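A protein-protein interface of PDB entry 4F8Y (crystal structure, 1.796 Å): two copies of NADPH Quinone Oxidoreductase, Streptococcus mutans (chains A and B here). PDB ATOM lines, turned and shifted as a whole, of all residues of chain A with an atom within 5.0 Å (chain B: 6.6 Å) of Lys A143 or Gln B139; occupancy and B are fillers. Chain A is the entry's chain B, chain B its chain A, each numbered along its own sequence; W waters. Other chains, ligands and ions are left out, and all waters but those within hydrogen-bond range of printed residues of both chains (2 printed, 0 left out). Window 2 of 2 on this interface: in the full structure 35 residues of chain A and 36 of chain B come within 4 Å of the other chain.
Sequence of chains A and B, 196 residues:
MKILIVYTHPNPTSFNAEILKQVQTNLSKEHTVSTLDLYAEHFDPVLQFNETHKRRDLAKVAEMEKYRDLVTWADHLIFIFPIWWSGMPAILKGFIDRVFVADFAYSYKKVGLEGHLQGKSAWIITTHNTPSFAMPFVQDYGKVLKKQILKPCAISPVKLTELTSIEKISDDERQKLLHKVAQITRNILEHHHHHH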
ATOM      1  N   MET A 135      30.849   8.484   6.581  1.00  0.00           N
ATOM      2  CA  MET A 135      29.806   9.233   5.891  1.00  0.00           C
ATOM      3  C   MET A 135      29.042  10.279   6.704  1.00  0.00           C
ATOM      4  O   MET A 135      28.598  11.281   6.153  1.00  0.00           O
ATOM      5  CB  MET A 135      28.840   8.273   5.208  1.00  0.00           C
ATOM      6  CG  MET A 135      29.393   7.688   3.924  1.00  0.00           C
ATOM      7  SD  MET A 135      29.769   8.951   2.690  1.00  0.00           S
ATOM      8  CE  MET A 135      31.484   9.285   3.040  1.00  0.00           C
ATOM      9  N   PRO A 136      28.856  10.040   8.010  1.00  0.00           N
ATOM     10  CA  PRO A 136      28.247  11.090   8.837  1.00  0.00           C
ATOM     11  C   PRO A 136      29.126  12.344   8.902  1.00  0.00           C
ATOM     12  O   PRO A 136      28.615  13.449   9.092  1.00  0.00           O
ATOM     13  CB  PRO A 136      28.157  10.436  10.218  1.00  0.00           C
ATOM     14  CG  PRO A 136      28.135   8.973   9.950  1.00  0.00           C
ATOM     15  CD  PRO A 136      28.968   8.756   8.729  1.00  0.00           C
ATOM     16  N   VAL A 138      30.980  13.756   6.477  1.00  0.00           N
ATOM     17  CA  VAL A 138      31.270  14.374   5.180  1.00  0.00           C
ATOM     18  C   VAL A 138      30.136  15.250   4.646  1.00  0.00           C
ATOM     19  O   VAL A 138      28.960  15.025   4.940  1.00  0.00           O
ATOM     20  CB  VAL A 138      31.624  13.331   4.093  1.00  0.00           C
ATOM     21  CG1 VAL A 138      32.850  12.526   4.485  1.00  0.00           C
ATOM     22  CG2 VAL A 138      30.441  12.433   3.828  1.00  0.00           C
ATOM     23  N   GLN A 139      30.518  16.240   3.841  1.00  0.00           N
ATOM     24  CA  GLN A 139      29.597  17.163   3.181  1.00  0.00           C
ATOM     25  C   GLN A 139      29.112  16.610   1.845  1.00  0.00           C
ATOM     26  O   GLN A 139      29.874  15.974   1.120  1.00  0.00           O
ATOM     27  CB  GLN A 139      30.303  18.494   2.921  1.00  0.00           C
ATOM     28  CG  GLN A 139      30.723  19.238   4.156  1.00  0.00           C
ATOM     29  CD  GLN A 139      29.639  20.144   4.658  1.00  0.00           C
ATOM     30  OE1 GLN A 139      29.002  20.853   3.881  1.00  0.00           O
ATOM     31  NE2 GLN A 139      29.412  20.128   5.963  1.00  0.00           N
ATOM     32  N   ASP A 140      27.849  16.872   1.528  1.00  0.00           N
ATOM     33  CA  ASP A 140      27.242  16.493   0.245  1.00  0.00           C
ATOM     34  C   ASP A 140      27.160  14.977   0.046  1.00  0.00           C
ATOM     35  O   ASP A 140      26.389  14.301   0.731  1.00  0.00           O
ATOM     36  CB  ASP A 140      27.960  17.170  -0.935  1.00  0.00           C
ATOM     37  CG  ASP A 140      27.146  17.125  -2.227  1.00  0.00           C
ATOM     38  OD1 ASP A 140      26.107  16.426  -2.278  1.00  0.00           O
ATOM     39  OD2 ASP A 140      27.542  17.801  -3.191  1.00  0.00           O
ATOM     40  N   TYR A 141      27.941  14.446  -0.892  1.00  0.00           N
ATOM     41  CA  TYR A 141      27.914  13.011  -1.174  1.00  0.00           C
ATOM     42  C   TYR A 141      26.493  12.526  -1.496  1.00  0.00           C
ATOM     43  O   TYR A 141      26.070  11.461  -1.054  1.00  0.00           O
ATOM     44  CB  TYR A 141      28.533  12.206  -0.016  1.00  0.00           C
ATOM     45  CG  TYR A 141      30.042  12.091  -0.089  1.00  0.00           C
ATOM     46  CD1 TYR A 141      30.647  10.919  -0.519  1.00  0.00           C
ATOM     47  CD2 TYR A 141      30.859  13.156   0.261  1.00  0.00           C
ATOM     48  CE1 TYR A 141      32.025  10.806  -0.593  1.00  0.00           C
ATOM     49  CE2 TYR A 141      32.248  13.058   0.187  1.00  0.00           C
ATOM     50  CZ  TYR A 141      32.825  11.878  -0.236  1.00  0.00           C
ATOM     51  OH  TYR A 141      34.201  11.765  -0.308  1.00  0.00           O
ATOM     52  N   GLY A 142      25.769  13.329  -2.275  1.00  0.00           N
ATOM     53  CA  GLY A 142      24.409  13.018  -2.668  1.00  0.00           C
ATOM     54  C   GLY A 142      23.368  13.784  -1.870  1.00  0.00           C
ATOM     55  O   GLY A 142      22.222  13.928  -2.303  1.00  0.00           O
ATOM     56  N   LYS A 143      23.765  14.280  -0.703  1.00  0.00           N
ATOM     57  CA  LYS A 143      22.835  14.956   0.194  1.00  0.00           C
ATOM     58  C   LYS A 143      22.419  16.352  -0.300  1.00  0.00           C
ATOM     59  O   LYS A 143      21.324  16.809   0.002  1.00  0.00           O
ATOM     60  CB  LYS A 143      23.404  15.022   1.620  1.00  0.00           C
ATOM     61  CG  LYS A 143      23.603  13.663   2.284  1.00  0.00           C
ATOM     62  CD  LYS A 143      23.994  13.795   3.752  1.00  0.00           C
ATOM     63  CE  LYS A 143      25.458  14.212   3.917  1.00  0.00           C
ATOM     64  NZ  LYS A 143      25.823  14.418   5.349  1.00  0.00           N
ATOM     65  N   VAL A 144      23.280  17.021  -1.057  1.00  0.00           N
ATOM     66  CA  VAL A 144      22.913  18.317  -1.617  1.00  0.00           C
ATOM     67  C   VAL A 144      21.804  18.164  -2.661  1.00  0.00           C
ATOM     68  O   VAL A 144      20.792  18.867  -2.605  1.00  0.00           O
ATOM     69  CB  VAL A 144      24.124  19.089  -2.201  1.00  0.00           C
ATOM     70  CG1 VAL A 144      23.651  20.255  -3.065  1.00  0.00           C
ATOM     71  CG2 VAL A 144      25.020  19.596  -1.079  1.00  0.00           C
ATOM     72  N   LEU A 145      21.979  17.240  -3.599  1.00  0.00           N
ATOM     73  CA  LEU A 145      20.943  16.985  -4.597  1.00  0.00           C
ATOM     74  C   LEU A 145      19.619  16.654  -3.913  1.00  0.00           C
ATOM     75  O   LEU A 145      18.569  17.193  -4.267  1.00  0.00           O
ATOM     76  CB  LEU A 145      21.345  15.838  -5.521  1.00  0.00           C
ATOM     77  CG  LEU A 145      20.286  15.307  -6.498  1.00  0.00           C
ATOM     78  CD1 LEU A 145      19.696  16.439  -7.334  1.00  0.00           C
ATOM     79  CD2 LEU A 145      20.874  14.229  -7.384  1.00  0.00           C
ATOM     80  N   LYS A 146      19.675  15.761  -2.931  1.00  0.00           N
ATOM     81  CA  LYS A 146      18.472  15.319  -2.245  1.00  0.00           C
ATOM     82  C   LYS A 146      17.868  16.435  -1.411  1.00  0.00           C
ATOM     83  O   LYS A 146      16.726  16.844  -1.640  1.00  0.00           O
ATOM     84  CB  LYS A 146      18.759  14.099  -1.362  1.00  0.00           C
ATOM     85  CG  LYS A 146      17.573  13.701  -0.489  1.00  0.00           C
ATOM     86  CD  LYS A 146      17.710  12.332   0.147  1.00  0.00           C
ATOM     87  CE  LYS A 146      16.724  12.215   1.311  1.00  0.00           C
ATOM     88  NZ  LYS A 146      16.264  10.824   1.555  1.00  0.00           N
ATOM     89  N   LYS A 147      18.657  16.931  -0.460  1.00  0.00           N
ATOM     90  CA  LYS A 147      18.174  17.813   0.594  1.00  0.00           C
ATOM     91  C   LYS A 147      18.009  19.266   0.156  1.00  0.00           C
ATOM     92  O   LYS A 147      17.123  19.972   0.645  1.00  0.00           O
ATOM     93  CB  LYS A 147      19.100  17.746   1.823  1.00  0.00           C
ATOM     94  CG  LYS A 147      19.151  16.392   2.518  1.00  0.00           C
ATOM     95  N   GLN A 148      18.859  19.712  -0.766  1.00  0.00           N
ATOM     96  CA  GLN A 148      18.930  21.129  -1.090  1.00  0.00           C
ATOM     97  C   GLN A 148      18.680  21.463  -2.564  1.00  0.00           C
ATOM     98  O   GLN A 148      18.758  22.637  -2.955  1.00  0.00           O
ATOM     99  CB  GLN A 148      20.259  21.696  -0.575  1.00  0.00           C
ATOM    100  CG  GLN A 148      20.513  21.243   0.872  1.00  0.00           C
ATOM    101  CD  GLN A 148      21.708  21.889   1.549  1.00  0.00           C
ATOM    102  OE1 GLN A 148      21.876  21.757   2.760  1.00  0.00           O
ATOM    103  NE2 GLN A 148      22.541  22.579   0.779  1.00  0.00           N
ATOM    104  N   LEU A 160      17.845   8.066  -1.226  1.00  0.00           N
ATOM    105  CA  LEU A 160      19.265   8.140  -1.551  1.00  0.00           C
ATOM    106  C   LEU A 160      20.004   6.830  -1.230  1.00  0.00           C
ATOM    107  O   LEU A 160      20.075   6.389  -0.079  1.00  0.00           O
ATOM    108  CB  LEU A 160      19.922   9.351  -0.870  1.00  0.00           C
ATOM    109  CG  LEU A 160      21.429   9.583  -1.010  1.00  0.00           C
ATOM    110  CD1 LEU A 160      21.939   9.354  -2.435  1.00  0.00           C
ATOM    111  CD2 LEU A 160      21.769  10.977  -0.531  1.00  0.00           C
ATOM    112  N   SER B  86      23.726  25.319  -3.885  1.00  0.00           N
ATOM    113  CA  SER B  86      24.533  24.968  -2.714  1.00  0.00           C
ATOM    114  C   SER B  86      26.027  24.783  -2.988  1.00  0.00           C
ATOM    115  O   SER B  86      26.785  24.455  -2.077  1.00  0.00           O
ATOM    116  CB  SER B  86      23.970  23.719  -2.043  1.00  0.00           C
ATOM    117  OG  SER B  86      22.574  23.846  -1.858  1.00  0.00           O
ATOM    118  N   GLY B  87      26.454  24.985  -4.234  1.00  0.00           N
ATOM    119  CA  GLY B  87      27.850  24.794  -4.573  1.00  0.00           C
ATOM    120  C   GLY B  87      28.371  25.528  -5.795  1.00  0.00           C
ATOM    121  O   GLY B  87      27.790  26.502  -6.265  1.00  0.00           O
ATOM    122  N   ALA B 134      22.601  30.313   8.947  1.00  0.00           N
ATOM    123  CA  ALA B 134      22.289  29.005   8.390  1.00  0.00           C
ATOM    124  C   ALA B 134      23.542  28.304   7.891  1.00  0.00           C
ATOM    125  O   ALA B 134      23.519  27.108   7.611  1.00  0.00           O
ATOM    126  CB  ALA B 134      21.283  29.143   7.267  1.00  0.00           C
ATOM    127  N   MET B 135      24.636  29.050   7.793  1.00  0.00           N
ATOM    128  CA  MET B 135      25.857  28.542   7.171  1.00  0.00           C
ATOM    129  C   MET B 135      26.458  27.301   7.845  1.00  0.00           C
ATOM    130  O   MET B 135      26.878  26.371   7.160  1.00  0.00           O
ATOM    131  CB  MET B 135      26.893  29.658   7.041  1.00  0.00           C
ATOM    132  CG  MET B 135      26.483  30.783   6.094  1.00  0.00           C
ATOM    133  SD  MET B 135      26.109  30.221   4.416  1.00  0.00           S
ATOM    134  CE  MET B 135      24.323  30.131   4.487  1.00  0.00           C
ATOM    135  N   PRO B 136      26.516  27.282   9.189  1.00  0.00           N
ATOM    136  CA  PRO B 136      27.003  26.061   9.845  1.00  0.00           C
ATOM    137  C   PRO B 136      26.141  24.815   9.568  1.00  0.00           C
ATOM    138  O   PRO B 136      26.558  23.707   9.904  1.00  0.00           O
ATOM    139  CB  PRO B 136      26.948  26.422  11.338  1.00  0.00           C
ATOM    140  CG  PRO B 136      27.064  27.904  11.373  1.00  0.00           C
ATOM    141  CD  PRO B 136      26.368  28.402  10.139  1.00  0.00           C
ATOM    142  N   PHE B 137      24.975  24.986   8.954  1.00  0.00           N
ATOM    143  CA  PHE B 137      23.990  23.905   8.897  1.00  0.00           C
ATOM    144  C   PHE B 137      23.702  23.390   7.494  1.00  0.00           C
ATOM    145  O   PHE B 137      23.318  22.235   7.315  1.00  0.00           O
ATOM    146  CB  PHE B 137      22.687  24.340   9.575  1.00  0.00           C
ATOM    147  CG  PHE B 137      22.851  24.662  11.026  1.00  0.00           C
ATOM    148  CD1 PHE B 137      22.974  23.645  11.963  1.00  0.00           C
ATOM    149  CD2 PHE B 137      22.899  25.975  11.458  1.00  0.00           C
ATOM    150  CE1 PHE B 137      23.133  23.931  13.300  1.00  0.00           C
ATOM    151  CE2 PHE B 137      23.055  26.268  12.792  1.00  0.00           C
ATOM    152  CZ  PHE B 137      23.173  25.243  13.719  1.00  0.00           C
ATOM    153  N   VAL B 138      23.878  24.248   6.499  1.00  0.00           N
ATOM    154  CA  VAL B 138      23.678  23.833   5.122  1.00  0.00           C
ATOM    155  C   VAL B 138      24.862  23.005   4.630  1.00  0.00           C
ATOM    156  O   VAL B 138      26.015  23.293   4.954  1.00  0.00           O
ATOM    157  CB  VAL B 138      23.505  25.041   4.201  1.00  0.00           C
ATOM    158  CG1 VAL B 138      22.160  25.711   4.454  1.00  0.00           C
ATOM    159  CG2 VAL B 138      24.651  26.013   4.402  1.00  0.00           C
ATOM    160  N   GLN B 139      24.572  21.973   3.852  1.00  0.00           N
ATOM    161  CA  GLN B 139      25.612  21.240   3.142  1.00  0.00           C
ATOM    162  C   GLN B 139      26.324  22.161   2.150  1.00  0.00           C
ATOM    163  O   GLN B 139      25.683  22.979   1.474  1.00  0.00           O
ATOM    164  CB  GLN B 139      25.008  20.043   2.408  1.00  0.00           C
ATOM    165  CG  GLN B 139      24.356  19.049   3.336  1.00  0.00           C
ATOM    166  CD  GLN B 139      25.375  18.269   4.113  1.00  0.00           C
ATOM    167  OE1 GLN B 139      26.240  17.632   3.534  1.00  0.00           O
ATOM    168  NE2 GLN B 139      25.288  18.316   5.435  1.00  0.00           N
ATOM    169  N   ASP B 140      27.650  22.027   2.084  1.00  0.00           N
ATOM    170  CA  ASP B 140      28.485  22.747   1.122  1.00  0.00           C
ATOM    171  C   ASP B 140      28.457  24.270   1.328  1.00  0.00           C
ATOM    172  O   ASP B 140      28.950  24.770   2.346  1.00  0.00           O
ATOM    173  CB  ASP B 140      28.115  22.362  -0.315  1.00  0.00           C
ATOM    174  CG  ASP B 140      29.198  22.707  -1.311  1.00  0.00           C
ATOM    175  OD1 ASP B 140      30.187  23.354  -0.915  1.00  0.00           O
ATOM    176  OD2 ASP B 140      29.060  22.336  -2.491  1.00  0.00           O
ATOM    177  N   TYR B 141      27.886  25.008   0.377  1.00  0.00           N
ATOM    178  CA  TYR B 141      28.008  26.475   0.377  1.00  0.00           C
ATOM    179  C   TYR B 141      29.468  26.937   0.514  1.00  0.00           C
ATOM    180  O   TYR B 141      29.785  27.818   1.325  1.00  0.00           O
ATOM    181  CB  TYR B 141      27.142  27.109   1.471  1.00  0.00           C
ATOM    182  CG  TYR B 141      25.697  27.294   1.072  1.00  0.00           C
ATOM    183  CD1 TYR B 141      25.202  28.550   0.746  1.00  0.00           C
ATOM    184  CD2 TYR B 141      24.829  26.215   1.018  1.00  0.00           C
ATOM    185  CE1 TYR B 141      23.876  28.725   0.378  1.00  0.00           C
ATOM    186  CE2 TYR B 141      23.505  26.381   0.651  1.00  0.00           C
ATOM    187  CZ  TYR B 141      23.038  27.638   0.330  1.00  0.00           C
ATOM    188  OH  TYR B 141      21.726  27.803  -0.032  1.00  0.00           O
ATOM    189  N   GLY B 142      30.347  26.347  -0.294  1.00  0.00           N
ATOM    190  CA  GLY B 142      31.762  26.679  -0.264  1.00  0.00           C
ATOM    191  C   GLY B 142      32.582  25.805   0.667  1.00  0.00           C
ATOM    192  O   GLY B 142      33.805  25.770   0.560  1.00  0.00           O
ATOM    193  N   LYS B 143      31.906  25.105   1.578  1.00  0.00           N
ATOM    194  CA  LYS B 143      32.563  24.207   2.528  1.00  0.00           C
ATOM    195  C   LYS B 143      33.148  22.942   1.883  1.00  0.00           C
ATOM    196  O   LYS B 143      34.140  22.410   2.367  1.00  0.00           O
ATOM    197  CB  LYS B 143      31.625  23.839   3.690  1.00  0.00           C
ATOM    198  CG  LYS B 143      31.309  24.994   4.625  1.00  0.00           C
ATOM    199  CD  LYS B 143      30.486  24.538   5.823  1.00  0.00           C
ATOM    200  CE  LYS B 143      29.063  24.159   5.420  1.00  0.00           C
ATOM    201  NZ  LYS B 143      28.211  23.801   6.585  1.00  0.00           N
ATOM    202  N   VAL B 144      32.543  22.454   0.806  1.00  0.00           N
ATOM    203  CA  VAL B 144      33.115  21.311   0.092  1.00  0.00           C
ATOM    204  C   VAL B 144      34.476  21.679  -0.517  1.00  0.00           C
ATOM    205  O   VAL B 144      35.475  21.024  -0.243  1.00  0.00           O
ATOM    206  CB  VAL B 144      32.145  20.729  -0.983  1.00  0.00           C
ATOM    207  CG1 VAL B 144      32.884  19.824  -1.956  1.00  0.00           C
ATOM    208  CG2 VAL B 144      31.000  19.977  -0.318  1.00  0.00           C
HETATM  209  O   HOH W   1      29.358  19.863  -3.329  1.00  0.00           O
HETATM  210  O   HOH W   2      20.457  24.550  -3.385  1.00  0.00           O
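NE2 of Gln A148 lies within hydrogen-bond range of OG of Ser B86 (2.9 Å). The side-chain amide oxygen of Gln B139 is in hydrogen-bond range of the backbone NH of Asp A140 (2.7 Å). The backbone NH (N) of Gln B139 lies within hydrogen-bond range of the side-chain amide oxygen (OE1) of Gln A148 (2.9 Å). The backbone NH (N) of Asp B140 is in hydrogen-bond range of the side-chain amide oxygen (OE1) of Gln A139.
The backbone carbonyl oxygen (O) of Met B135 is in hydrogen-bond range of the side-chain amino group (NZ) of Lys B143, 3.0 Å away. OD1 of Asp B140 sits at hydrogen-bond distance from N of Gly B142, 3.1 Å away. The backbone NH of Lys B143 lies within hydrogen-bond range of the side-chain carboxylate of Asp B140, 3.5 Å away. N of Val B144 sits at hydrogen-bond distance from OD1 of Asp B140, at 3.1 Å. OD1 of Asp A140 sits at hydrogen-bond distance from N of Gly A142 (3.1 Å). OD1 of Asp A140 lies within hydrogen-bond range of N of Val A144, 3.1 Å away.
OE1 of Gln B139 touches CA of Gln A139 (3.4 Å). CE of Lys B143 touches OE1 of Gln A139 (3.6 Å). Gln A139 touches Val B144 (CB to CG2, 3.6 Å). Gln B139 touches Lys A143 (OE1 to CE, 3.5 Å). CG1 of Val A144 touches CB of Ser B86, at 3.6 Å. Gln B139 touches Val A144 (CB to CG2, 3.5 Å). Val B138 touches Gln A148 (CA to OE1, 3.6 Å). Tyr B141 touches Gln A148 (CE2 to NE2, 3.9 Å).
Lys A143 touches just one residue of chain B: Gln B139. Printed residues of chain A within 4 Å of Ser B86: Val A144 and Gln A148. Ala B134 touches none of the printed residues of chain A. Gln B139 touches just these residues of chain A: Gln A139 (3.4 Å), Asp A140 (2.7 Å), Lys A143 (3.5 Å), Val A144 (3.5 Å) and Gln A148 (2.9 Å). Of the printed residues of chain A, Lys B143 touches Gln A139. The nearest residue of chain A that does not touch Gln B139 is Val A138 (4.02 Å).
Of the 14 printed residues of chain A, 5 touch a printed residue of chain B. Among the printed residues, no Asp or Glu carboxylate lies within 4 Å of a Lys or Arg side-chain nitrogen of the other chain.
Gln B139 touches its own counterpart, Gln A139. Gln A139 touches Asp B140, and with the chains exchanged Asp A140 touches Gln B139. Gln A139 touches Lys B143, and with the chains exchanged Lys A143 touches Gln B139. Gln A139 touches Val B144, and with the chains exchanged Val A144 touches Gln B139. 9 positions are printed for both chains. Of the 12 pairs that touch across the chains among the printed residues, 7 have their exchanged pair printed and touching as well.
Water W2 lies within hydrogen-bond range of the backbone carbonyl oxygen of Gln A148 (2.6 Å) and the side-chain hydroxyl of Ser B86 (2.7 Å). Water W1 bridges OD2 of Asp B140 (2.6 Å) and OD2 of Asp A140 (2.8 Å).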
